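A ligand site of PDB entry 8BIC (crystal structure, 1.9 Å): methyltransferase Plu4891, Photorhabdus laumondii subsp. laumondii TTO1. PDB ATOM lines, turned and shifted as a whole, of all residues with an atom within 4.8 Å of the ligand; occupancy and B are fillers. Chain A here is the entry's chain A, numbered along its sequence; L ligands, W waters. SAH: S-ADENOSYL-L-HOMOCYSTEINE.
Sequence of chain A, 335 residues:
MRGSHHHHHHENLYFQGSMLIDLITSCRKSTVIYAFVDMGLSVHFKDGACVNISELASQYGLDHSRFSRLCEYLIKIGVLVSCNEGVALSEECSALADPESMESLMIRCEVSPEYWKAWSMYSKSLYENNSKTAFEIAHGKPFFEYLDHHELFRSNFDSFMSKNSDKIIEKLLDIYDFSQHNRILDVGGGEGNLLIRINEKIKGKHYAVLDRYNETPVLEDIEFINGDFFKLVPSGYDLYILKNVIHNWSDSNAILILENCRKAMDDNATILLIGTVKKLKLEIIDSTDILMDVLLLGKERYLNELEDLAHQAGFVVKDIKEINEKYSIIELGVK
O of Lys 243 lies within hydrogen-bond range of N of the ligand, at 2.7 Å.
OD1 of Asp 211 lies within hydrogen-bond range of O2' of the ligand, at 2.5 Å.
A nitrogen (N6) of the ligand lies within hydrogen-bond range of the side-chain carboxylate (OD2) of Asp 228 (2.9 Å).
N of the ligand sits at hydrogen-bond distance from O of Gly 188, 2.8 Å away.
OXT of the ligand is in salt-bridge range of NZ of Lys 243, 2.8 Å away.
The backbone NH of Phe 229 lies within hydrogen-bond range of a nitrogen (N1) of the ligand (3.1 Å).
Water W3 lies within hydrogen-bond range of the side-chain hydroxyl (OG) of Ser 165, an oxygen (O) of the ligand and the backbone carbonyl oxygen (O) of Met 161.
Water W4 lies within hydrogen-bond range of an oxygen (O) of the ligand (2.8 Å), the side-chain amide nitrogen (ND2) of Asn 244 (3.0 Å), the side-chain sulfur (SD) of Met 161 (3.1 Å) and the side-chain amino group (NZ) of Lys 243 (3.4 Å).
Water W5 bridges an oxygen (O3') of the ligand and the side-chain carboxylate of Asp 158.
Water W7 lies within hydrogen-bond range of O4' of the ligand, ND2 of Asn 248 and NE1 of Trp 249.
Water W6 lies within hydrogen-bond range of OD1 of Asp 158 (2.7 Å) and O2' of the ligand (2.9 Å).
Water W1 lies within hydrogen-bond range of OD1 of Asp 186, N of Lys 243 and N of the ligand.
An oxygen (O) of the ligand sits close to the backbone carbonyl oxygen (O) of Met 161, at 3.2 Å.
A sulfur (SD) of the ligand lies close to the backbone carbonyl oxygen (O) of Asn 244, at 3.7 Å.
Phe 144 touches the ligand (CE1 to C2', 3.6 Å).
Ser 165 touches the ligand.
Gly 189 touches the ligand (CA to N, 3.8 Å).
Gly 190 touches the ligand.
Arg 212 touches the ligand (CD to C6, 3.5 Å).
CD2 of Phe 230 touches N6 of the ligand (3.6 Å).
Asn 248 touches the ligand.
Trp 249 touches the ligand.
Hydrophobic or aromatic side chains that line the ligand: Phe 144, Met 161, Phe 229, Phe 230 and Trp 249.
Of the 22 residues printed, 15 come within 4 Å of the ligand.
The side-chain carboxylate (OD2) of Asp 211 lies within hydrogen-bond range of the backbone NH (N) of Gly 190, 2.7 Å away.
N of Gly 227 sits at hydrogen-bond distance from O of Asp 211 (3.1 Å).
The side-chain amino group (NZ) of Lys 243 is in hydrogen-bond range of the side-chain hydroxyl (OG) of Ser 165, 2.9 Å away.
N of Gly 189 lies within hydrogen-bond range of O of Leu 210, 3.4 Å away.
O of Phe 144 is in hydrogen-bond range of NH1 of Arg 212 (3.2 Å).
NZ of Lys 243 sits close to ND2 of Asn 244 (3.4 Å).
N of Gly 188 sits at hydrogen-bond distance from O of Leu 210 (2.7 Å).
The side-chain carboxylate (OD2) of Asp 228 is in hydrogen-bond range of the backbone NH (N) of Phe 230 (3.0 Å).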
ATOM      1  N   PHE A 144       3.060  -5.493  11.816  1.00  0.00           N
ATOM      2  CA  PHE A 144       2.805  -6.965  11.773  1.00  0.00           C
ATOM      3  C   PHE A 144       1.321  -7.231  11.506  1.00  0.00           C
ATOM      4  O   PHE A 144       1.027  -8.227  10.815  1.00  0.00           O
ATOM      5  CB  PHE A 144       3.374  -7.632  13.026  1.00  0.00           C
ATOM      6  CG  PHE A 144       4.873  -7.595  13.084  1.00  0.00           C
ATOM      7  CD1 PHE A 144       5.627  -8.227  12.104  1.00  0.00           C
ATOM      8  CD2 PHE A 144       5.533  -6.927  14.099  1.00  0.00           C
ATOM      9  CE1 PHE A 144       7.013  -8.176  12.137  1.00  0.00           C
ATOM     10  CE2 PHE A 144       6.917  -6.884  14.138  1.00  0.00           C
ATOM     11  CZ  PHE A 144       7.662  -7.514  13.159  1.00  0.00           C
ATOM     12  N   PHE A 157       8.865  -9.908   2.683  1.00  0.00           N
ATOM     13  CA  PHE A 157       9.465  -9.667   4.024  1.00  0.00           C
ATOM     14  C   PHE A 157       9.912 -11.002   4.652  1.00  0.00           C
ATOM     15  O   PHE A 157      11.079 -11.092   5.110  1.00  0.00           O
ATOM     16  CB  PHE A 157       8.492  -8.941   4.955  1.00  0.00           C
ATOM     17  CG  PHE A 157       9.029  -8.726   6.347  1.00  0.00           C
ATOM     18  CD1 PHE A 157       9.835  -7.634   6.642  1.00  0.00           C
ATOM     19  CD2 PHE A 157       8.753  -9.626   7.362  1.00  0.00           C
ATOM     20  CE1 PHE A 157      10.333  -7.437   7.919  1.00  0.00           C
ATOM     21  CE2 PHE A 157       9.261  -9.431   8.638  1.00  0.00           C
ATOM     22  CZ  PHE A 157      10.054  -8.341   8.912  1.00  0.00           C
ATOM     23  N   ASP A 158       9.022 -12.000   4.672  1.00  0.00           N
ATOM     24  CA  ASP A 158       9.279 -13.313   5.332  1.00  0.00           C
ATOM     25  C   ASP A 158      10.472 -13.994   4.642  1.00  0.00           C
ATOM     26  O   ASP A 158      11.332 -14.547   5.353  1.00  0.00           O
ATOM     27  CB  ASP A 158       8.022 -14.202   5.340  1.00  0.00           C
ATOM     28  CG  ASP A 158       6.964 -13.821   6.368  1.00  0.00           C
ATOM     29  OD1 ASP A 158       7.268 -13.046   7.304  1.00  0.00           O
ATOM     30  OD2 ASP A 158       5.829 -14.318   6.233  1.00  0.00           O
ATOM     31  N   MET A 161      13.735 -12.220   5.575  1.00  0.00           N
ATOM     32  CA  MET A 161      14.124 -12.675   6.925  1.00  0.00           C
ATOM     33  C   MET A 161      14.773 -14.062   6.827  1.00  0.00           C
ATOM     34  O   MET A 161      15.826 -14.262   7.463  1.00  0.00           O
ATOM     35  CB  MET A 161      12.921 -12.710   7.878  1.00  0.00           C
ATOM     36  CG  MET A 161      12.321 -11.340   8.164  1.00  0.00           C
ATOM     37  SD  MET A 161      13.418 -10.203   9.046  1.00  0.00           S
ATOM     38  CE  MET A 161      13.988  -9.160   7.708  1.00  0.00           C
ATOM     39  N   SER A 162      14.217 -14.975   6.031  1.00  0.00           N
ATOM     40  CA  SER A 162      14.730 -16.362   5.836  1.00  0.00           C
ATOM     41  C   SER A 162      16.157 -16.327   5.282  1.00  0.00           C
ATOM     42  O   SER A 162      17.002 -17.107   5.779  1.00  0.00           O
ATOM     43  CB  SER A 162      13.817 -17.176   4.968  1.00  0.00           C
ATOM     44  OG  SER A 162      12.633 -17.532   5.677  1.00  0.00           O
ATOM     45  N   SER A 165      18.840 -15.519   7.895  1.00  0.00           N
ATOM     46  CA  SER A 165      19.212 -16.734   8.677  1.00  0.00           C
ATOM     47  C   SER A 165      20.242 -17.547   7.893  1.00  0.00           C
ATOM     48  O   SER A 165      21.170 -18.079   8.515  1.00  0.00           O
ATOM     49  CB  SER A 165      17.999 -17.569   9.027  1.00  0.00           C
ATOM     50  OG  SER A 165      17.255 -16.971  10.079  1.00  0.00           O
ATOM     51  N   ASP A 186      11.562 -21.697  18.222  1.00  0.00           N
ATOM     52  CA  ASP A 186      11.953 -20.459  17.487  1.00  0.00           C
ATOM     53  C   ASP A 186      10.832 -19.431  17.701  1.00  0.00           C
ATOM     54  O   ASP A 186       9.808 -19.515  17.005  1.00  0.00           O
ATOM     55  CB  ASP A 186      12.206 -20.768  16.014  1.00  0.00           C
ATOM     56  CG  ASP A 186      12.917 -19.676  15.232  1.00  0.00           C
ATOM     57  OD1 ASP A 186      13.253 -18.634  15.813  1.00  0.00           O
ATOM     58  OD2 ASP A 186      13.140 -19.901  14.026  1.00  0.00           O
ATOM     59  N   GLY A 188       8.983 -16.190  17.265  1.00  0.00           N
ATOM     60  CA  GLY A 188       8.929 -15.231  16.147  1.00  0.00           C
ATOM     61  C   GLY A 188       9.809 -15.669  14.988  1.00  0.00           C
ATOM     62  O   GLY A 188      10.435 -14.804  14.371  1.00  0.00           O
ATOM     63  N   GLY A 189       9.821 -16.969  14.685  1.00  0.00           N
ATOM     64  CA  GLY A 189      10.721 -17.588  13.675  1.00  0.00           C
ATOM     65  C   GLY A 189      10.228 -17.441  12.250  1.00  0.00           C
ATOM     66  O   GLY A 189      10.981 -17.836  11.329  1.00  0.00           O
ATOM     67  N   GLY A 190       9.012 -16.917  12.042  1.00  0.00           N
ATOM     68  CA  GLY A 190       8.443 -16.698  10.691  1.00  0.00           C
ATOM     69  C   GLY A 190       8.344 -18.006   9.908  1.00  0.00           C
ATOM     70  O   GLY A 190       7.666 -18.926  10.391  1.00  0.00           O
ATOM     71  N   LEU A 210       7.103 -20.497  16.648  1.00  0.00           N
ATOM     72  CA  LEU A 210       5.957 -19.667  17.113  1.00  0.00           C
ATOM     73  C   LEU A 210       5.930 -18.364  16.312  1.00  0.00           C
ATOM     74  O   LEU A 210       6.931 -17.629  16.343  1.00  0.00           O
ATOM     75  CB  LEU A 210       6.091 -19.370  18.613  1.00  0.00           C
ATOM     76  CG  LEU A 210       5.031 -18.423  19.183  1.00  0.00           C
ATOM     77  CD1 LEU A 210       3.653 -19.058  19.174  1.00  0.00           C
ATOM     78  CD2 LEU A 210       5.406 -17.967  20.582  1.00  0.00           C
ATOM     79  N   ASP A 211       4.815 -18.103  15.626  1.00  0.00           N
ATOM     80  CA  ASP A 211       4.594 -16.838  14.862  1.00  0.00           C
ATOM     81  C   ASP A 211       3.103 -16.695  14.544  1.00  0.00           C
ATOM     82  O   ASP A 211       2.310 -17.577  14.934  1.00  0.00           O
ATOM     83  CB  ASP A 211       5.469 -16.801  13.604  1.00  0.00           C
ATOM     84  CG  ASP A 211       5.954 -15.415  13.229  1.00  0.00           C
ATOM     85  OD1 ASP A 211       5.090 -14.528  13.029  1.00  0.00           O
ATOM     86  OD2 ASP A 211       7.185 -15.228  13.136  1.00  0.00           O
ATOM     87  N   ARG A 212       2.748 -15.610  13.863  1.00  0.00           N
ATOM     88  CA  ARG A 212       1.364 -15.296  13.428  1.00  0.00           C
ATOM     89  C   ARG A 212       1.229 -15.685  11.957  1.00  0.00           C
ATOM     90  O   ARG A 212       1.993 -15.138  11.130  1.00  0.00           O
ATOM     91  CB  ARG A 212       1.074 -13.812  13.686  1.00  0.00           C
ATOM     92  CG  ARG A 212       1.471 -13.349  15.084  1.00  0.00           C
ATOM     93  CD  ARG A 212       1.280 -11.866  15.299  1.00  0.00           C
ATOM     94  NE  ARG A 212      -0.089 -11.467  14.975  1.00  0.00           N
ATOM     95  CZ  ARG A 212      -0.477 -10.878  13.847  1.00  0.00           C
ATOM     96  NH1 ARG A 212       0.405 -10.572  12.903  1.00  0.00           N
ATOM     97  NH2 ARG A 212      -1.750 -10.580  13.681  1.00  0.00           N
ATOM     98  N   GLY A 227       0.356 -18.503  17.098  1.00  0.00           N
ATOM     99  CA  GLY A 227       0.104 -17.897  18.408  1.00  0.00           C
ATOM    100  C   GLY A 227       0.414 -16.410  18.436  1.00  0.00           C
ATOM    101  O   GLY A 227       0.351 -15.768  17.370  1.00  0.00           O
ATOM    102  N   ASP A 228       0.737 -15.896  19.617  1.00  0.00           N
ATOM    103  CA  ASP A 228       0.990 -14.451  19.872  1.00  0.00           C
ATOM    104  C   ASP A 228       1.822 -14.366  21.149  1.00  0.00           C
ATOM    105  O   ASP A 228       1.268 -14.636  22.218  1.00  0.00           O
ATOM    106  CB  ASP A 228      -0.339 -13.703  19.958  1.00  0.00           C
ATOM    107  CG  ASP A 228      -0.236 -12.225  20.286  1.00  0.00           C
ATOM    108  OD1 ASP A 228      -1.286 -11.549  20.247  1.00  0.00           O
ATOM    109  OD2 ASP A 228       0.878 -11.767  20.596  1.00  0.00           O
ATOM    110  N   PHE A 229       3.116 -14.026  21.054  1.00  0.00           N
ATOM    111  CA  PHE A 229       4.066 -14.063  22.204  1.00  0.00           C
ATOM    112  C   PHE A 229       3.737 -12.974  23.229  1.00  0.00           C
ATOM    113  O   PHE A 229       4.403 -12.946  24.296  1.00  0.00           O
ATOM    114  CB  PHE A 229       5.531 -14.053  21.758  1.00  0.00           C
ATOM    115  CG  PHE A 229       5.982 -12.987  20.784  1.00  0.00           C
ATOM    116  CD1 PHE A 229       6.857 -13.315  19.763  1.00  0.00           C
ATOM    117  CD2 PHE A 229       5.601 -11.668  20.923  1.00  0.00           C
ATOM    118  CE1 PHE A 229       7.321 -12.352  18.873  1.00  0.00           C
ATOM    119  CE2 PHE A 229       6.055 -10.703  20.034  1.00  0.00           C
ATOM    120  CZ  PHE A 229       6.914 -11.048  19.005  1.00  0.00           C
ATOM    121  N   PHE A 230       2.754 -12.108  22.956  1.00  0.00           N
ATOM    122  CA  PHE A 230       2.222 -11.124  23.931  1.00  0.00           C
ATOM    123  C   PHE A 230       1.152 -11.783  24.820  1.00  0.00           C
ATOM    124  O   PHE A 230       0.993 -11.338  25.963  1.00  0.00           O
ATOM    125  CB  PHE A 230       1.666  -9.889  23.230  1.00  0.00           C
ATOM    126  CG  PHE A 230       2.714  -9.006  22.606  1.00  0.00           C
ATOM    127  CD1 PHE A 230       3.694  -8.400  23.387  1.00  0.00           C
ATOM    128  CD2 PHE A 230       2.738  -8.786  21.232  1.00  0.00           C
ATOM    129  CE1 PHE A 230       4.665  -7.591  22.815  1.00  0.00           C
ATOM    130  CE2 PHE A 230       3.719  -7.979  20.659  1.00  0.00           C
ATOM    131  CZ  PHE A 230       4.665  -7.387  21.447  1.00  0.00           C
ATOM    132  N   LYS A 243      15.502 -14.559  17.536  1.00  0.00           N
ATOM    133  CA  LYS A 243      16.372 -13.982  16.476  1.00  0.00           C
ATOM    134  C   LYS A 243      15.664 -12.789  15.817  1.00  0.00           C
ATOM    135  O   LYS A 243      14.563 -12.980  15.260  1.00  0.00           O
ATOM    136  CB  LYS A 243      16.752 -15.031  15.432  1.00  0.00           C
ATOM    137  CG  LYS A 243      17.761 -14.565  14.395  1.00  0.00           C
ATOM    138  CD  LYS A 243      18.088 -15.622  13.360  1.00  0.00           C
ATOM    139  CE  LYS A 243      18.752 -15.037  12.131  1.00  0.00           C
ATOM    140  NZ  LYS A 243      17.758 -14.398  11.235  1.00  0.00           N
ATOM    141  N   ASN A 244      16.290 -11.606  15.874  1.00  0.00           N
ATOM    142  CA  ASN A 244      15.813 -10.368  15.211  1.00  0.00           C
ATOM    143  C   ASN A 244      14.365 -10.084  15.644  1.00  0.00           C
ATOM    144  O   ASN A 244      13.549  -9.723  14.778  1.00  0.00           O
ATOM    145  CB  ASN A 244      15.968 -10.479  13.690  1.00  0.00           C
ATOM    146  CG  ASN A 244      17.427 -10.576  13.271  1.00  0.00           C
ATOM    147  OD1 ASN A 244      18.305 -10.126  13.992  1.00  0.00           O
ATOM    148  ND2 ASN A 244      17.682 -11.157  12.108  1.00  0.00           N
ATOM    149  N   VAL A 245      14.065 -10.250  16.940  1.00  0.00           N
ATOM    150  CA  VAL A 245      12.713  -9.992  17.526  1.00  0.00           C
ATOM    151  C   VAL A 245      12.787  -8.742  18.410  1.00  0.00           C
ATOM    152  O   VAL A 245      12.017  -7.794  18.162  1.00  0.00           O
ATOM    153  CB  VAL A 245      12.195 -11.213  18.302  1.00  0.00           C
ATOM    154  CG1 VAL A 245      10.926 -10.923  19.081  1.00  0.00           C
ATOM    155  CG2 VAL A 245      11.974 -12.407  17.373  1.00  0.00           C
ATOM    156  N   ASN A 248      12.521  -5.090  17.329  1.00  0.00           N
ATOM    157  CA  ASN A 248      11.215  -4.690  16.743  1.00  0.00           C
ATOM    158  C   ASN A 248      10.330  -3.990  17.779  1.00  0.00           C
ATOM    159  O   ASN A 248       9.205  -3.597  17.408  1.00  0.00           O
ATOM    160  CB  ASN A 248      10.431  -5.898  16.207  1.00  0.00           C
ATOM    161  CG  ASN A 248      11.033  -6.566  14.996  1.00  0.00           C
ATOM    162  OD1 ASN A 248      11.917  -6.031  14.331  1.00  0.00           O
ATOM    163  ND2 ASN A 248      10.505  -7.737  14.683  1.00  0.00           N
ATOM    164  N   TRP A 249      10.764  -3.868  19.042  1.00  0.00           N
ATOM    165  CA  TRP A 249       9.827  -3.542  20.160  1.00  0.00           C
ATOM    166  C   TRP A 249      10.390  -2.471  21.094  1.00  0.00           C
ATOM    167  O   TRP A 249      11.603  -2.436  21.295  1.00  0.00           O
ATOM    168  CB  TRP A 249       9.469  -4.824  20.929  1.00  0.00           C
ATOM    169  CG  TRP A 249       8.830  -5.850  20.051  1.00  0.00           C
ATOM    170  CD1 TRP A 249       9.408  -6.995  19.572  1.00  0.00           C
ATOM    171  CD2 TRP A 249       7.525  -5.782  19.449  1.00  0.00           C
ATOM    172  NE1 TRP A 249       8.545  -7.652  18.754  1.00  0.00           N
ATOM    173  CE2 TRP A 249       7.375  -6.933  18.659  1.00  0.00           C
ATOM    174  CE3 TRP A 249       6.471  -4.867  19.519  1.00  0.00           C
ATOM    175  CZ2 TRP A 249       6.203  -7.201  17.938  1.00  0.00           C
ATOM    176  CZ3 TRP A 249       5.313  -5.126  18.813  1.00  0.00           C
ATOM    177  CH2 TRP A 249       5.186  -6.279  18.042  1.00  0.00           C
HETATM  178  N   SAH L   1      13.189 -14.683  13.716  1.00  0.00           N
HETATM  179  CA  SAH L   1      13.036 -14.495  12.243  1.00  0.00           C
HETATM  180  CB  SAH L   1      12.069 -13.349  11.890  1.00  0.00           C
HETATM  181  CG  SAH L   1      12.433 -12.002  12.523  1.00  0.00           C
HETATM  182  SD  SAH L   1      11.262 -10.689  12.089  1.00  0.00           S
HETATM  183  C   SAH L   1      14.407 -14.192  11.641  1.00  0.00           C
HETATM  184  O   SAH L   1      14.590 -14.340  10.442  1.00  0.00           O
HETATM  185  OXT SAH L   1      15.320 -13.816  12.391  1.00  0.00           O
HETATM  186  C5' SAH L   1      10.170 -10.679  13.522  1.00  0.00           C
HETATM  187  C4' SAH L   1       9.205 -11.842  13.558  1.00  0.00           C
HETATM  188  O4' SAH L   1       8.354 -11.717  14.718  1.00  0.00           O
HETATM  189  C3' SAH L   1       8.276 -11.966  12.339  1.00  0.00           C
HETATM  190  O3' SAH L   1       8.329 -13.275  11.788  1.00  0.00           O
HETATM  191  C2' SAH L   1       6.887 -11.644  12.916  1.00  0.00           C
HETATM  192  O2' SAH L   1       5.823 -12.262  12.248  1.00  0.00           O
HETATM  193  C1' SAH L   1       7.062 -12.152  14.346  1.00  0.00           C
HETATM  194  N9  SAH L   1       6.087 -11.619  15.276  1.00  0.00           N
HETATM  195  C8  SAH L   1       5.680 -10.304  15.388  1.00  0.00           C
HETATM  196  N7  SAH L   1       4.762 -10.127  16.303  1.00  0.00           N
HETATM  197  C5  SAH L   1       4.533 -11.399  16.819  1.00  0.00           C
HETATM  198  C6  SAH L   1       3.667 -11.866  17.824  1.00  0.00           C
HETATM  199  N6  SAH L   1       2.834 -11.089  18.509  1.00  0.00           N
HETATM  200  N1  SAH L   1       3.688 -13.195  18.112  1.00  0.00           N
HETATM  201  C2  SAH L   1       4.529 -13.972  17.412  1.00  0.00           C
HETATM  202  N3  SAH L   1       5.382 -13.648  16.451  1.00  0.00           N
HETATM  203  C4  SAH L   1       5.342 -12.326  16.199  1.00  0.00           C
HETATM  204  O   HOH W   1      13.235 -16.014  16.427  1.00  0.00           O
HETATM  205  O   HOH W   2      14.345 -17.220  13.610  1.00  0.00           O
HETATM  206  O   HOH W   3      14.697 -16.892   9.459  1.00  0.00           O
HETATM  207  O   HOH W   4      15.870 -11.956   9.860  1.00  0.00           O
HETATM  208  O   HOH W   5       9.392 -13.467   9.210  1.00  0.00           O
HETATM  209  O   HOH W   6       5.644 -12.781   9.383  1.00  0.00           O
HETATM  210  O   HOH W   7       8.928  -9.523  16.391  1.00  0.00           O
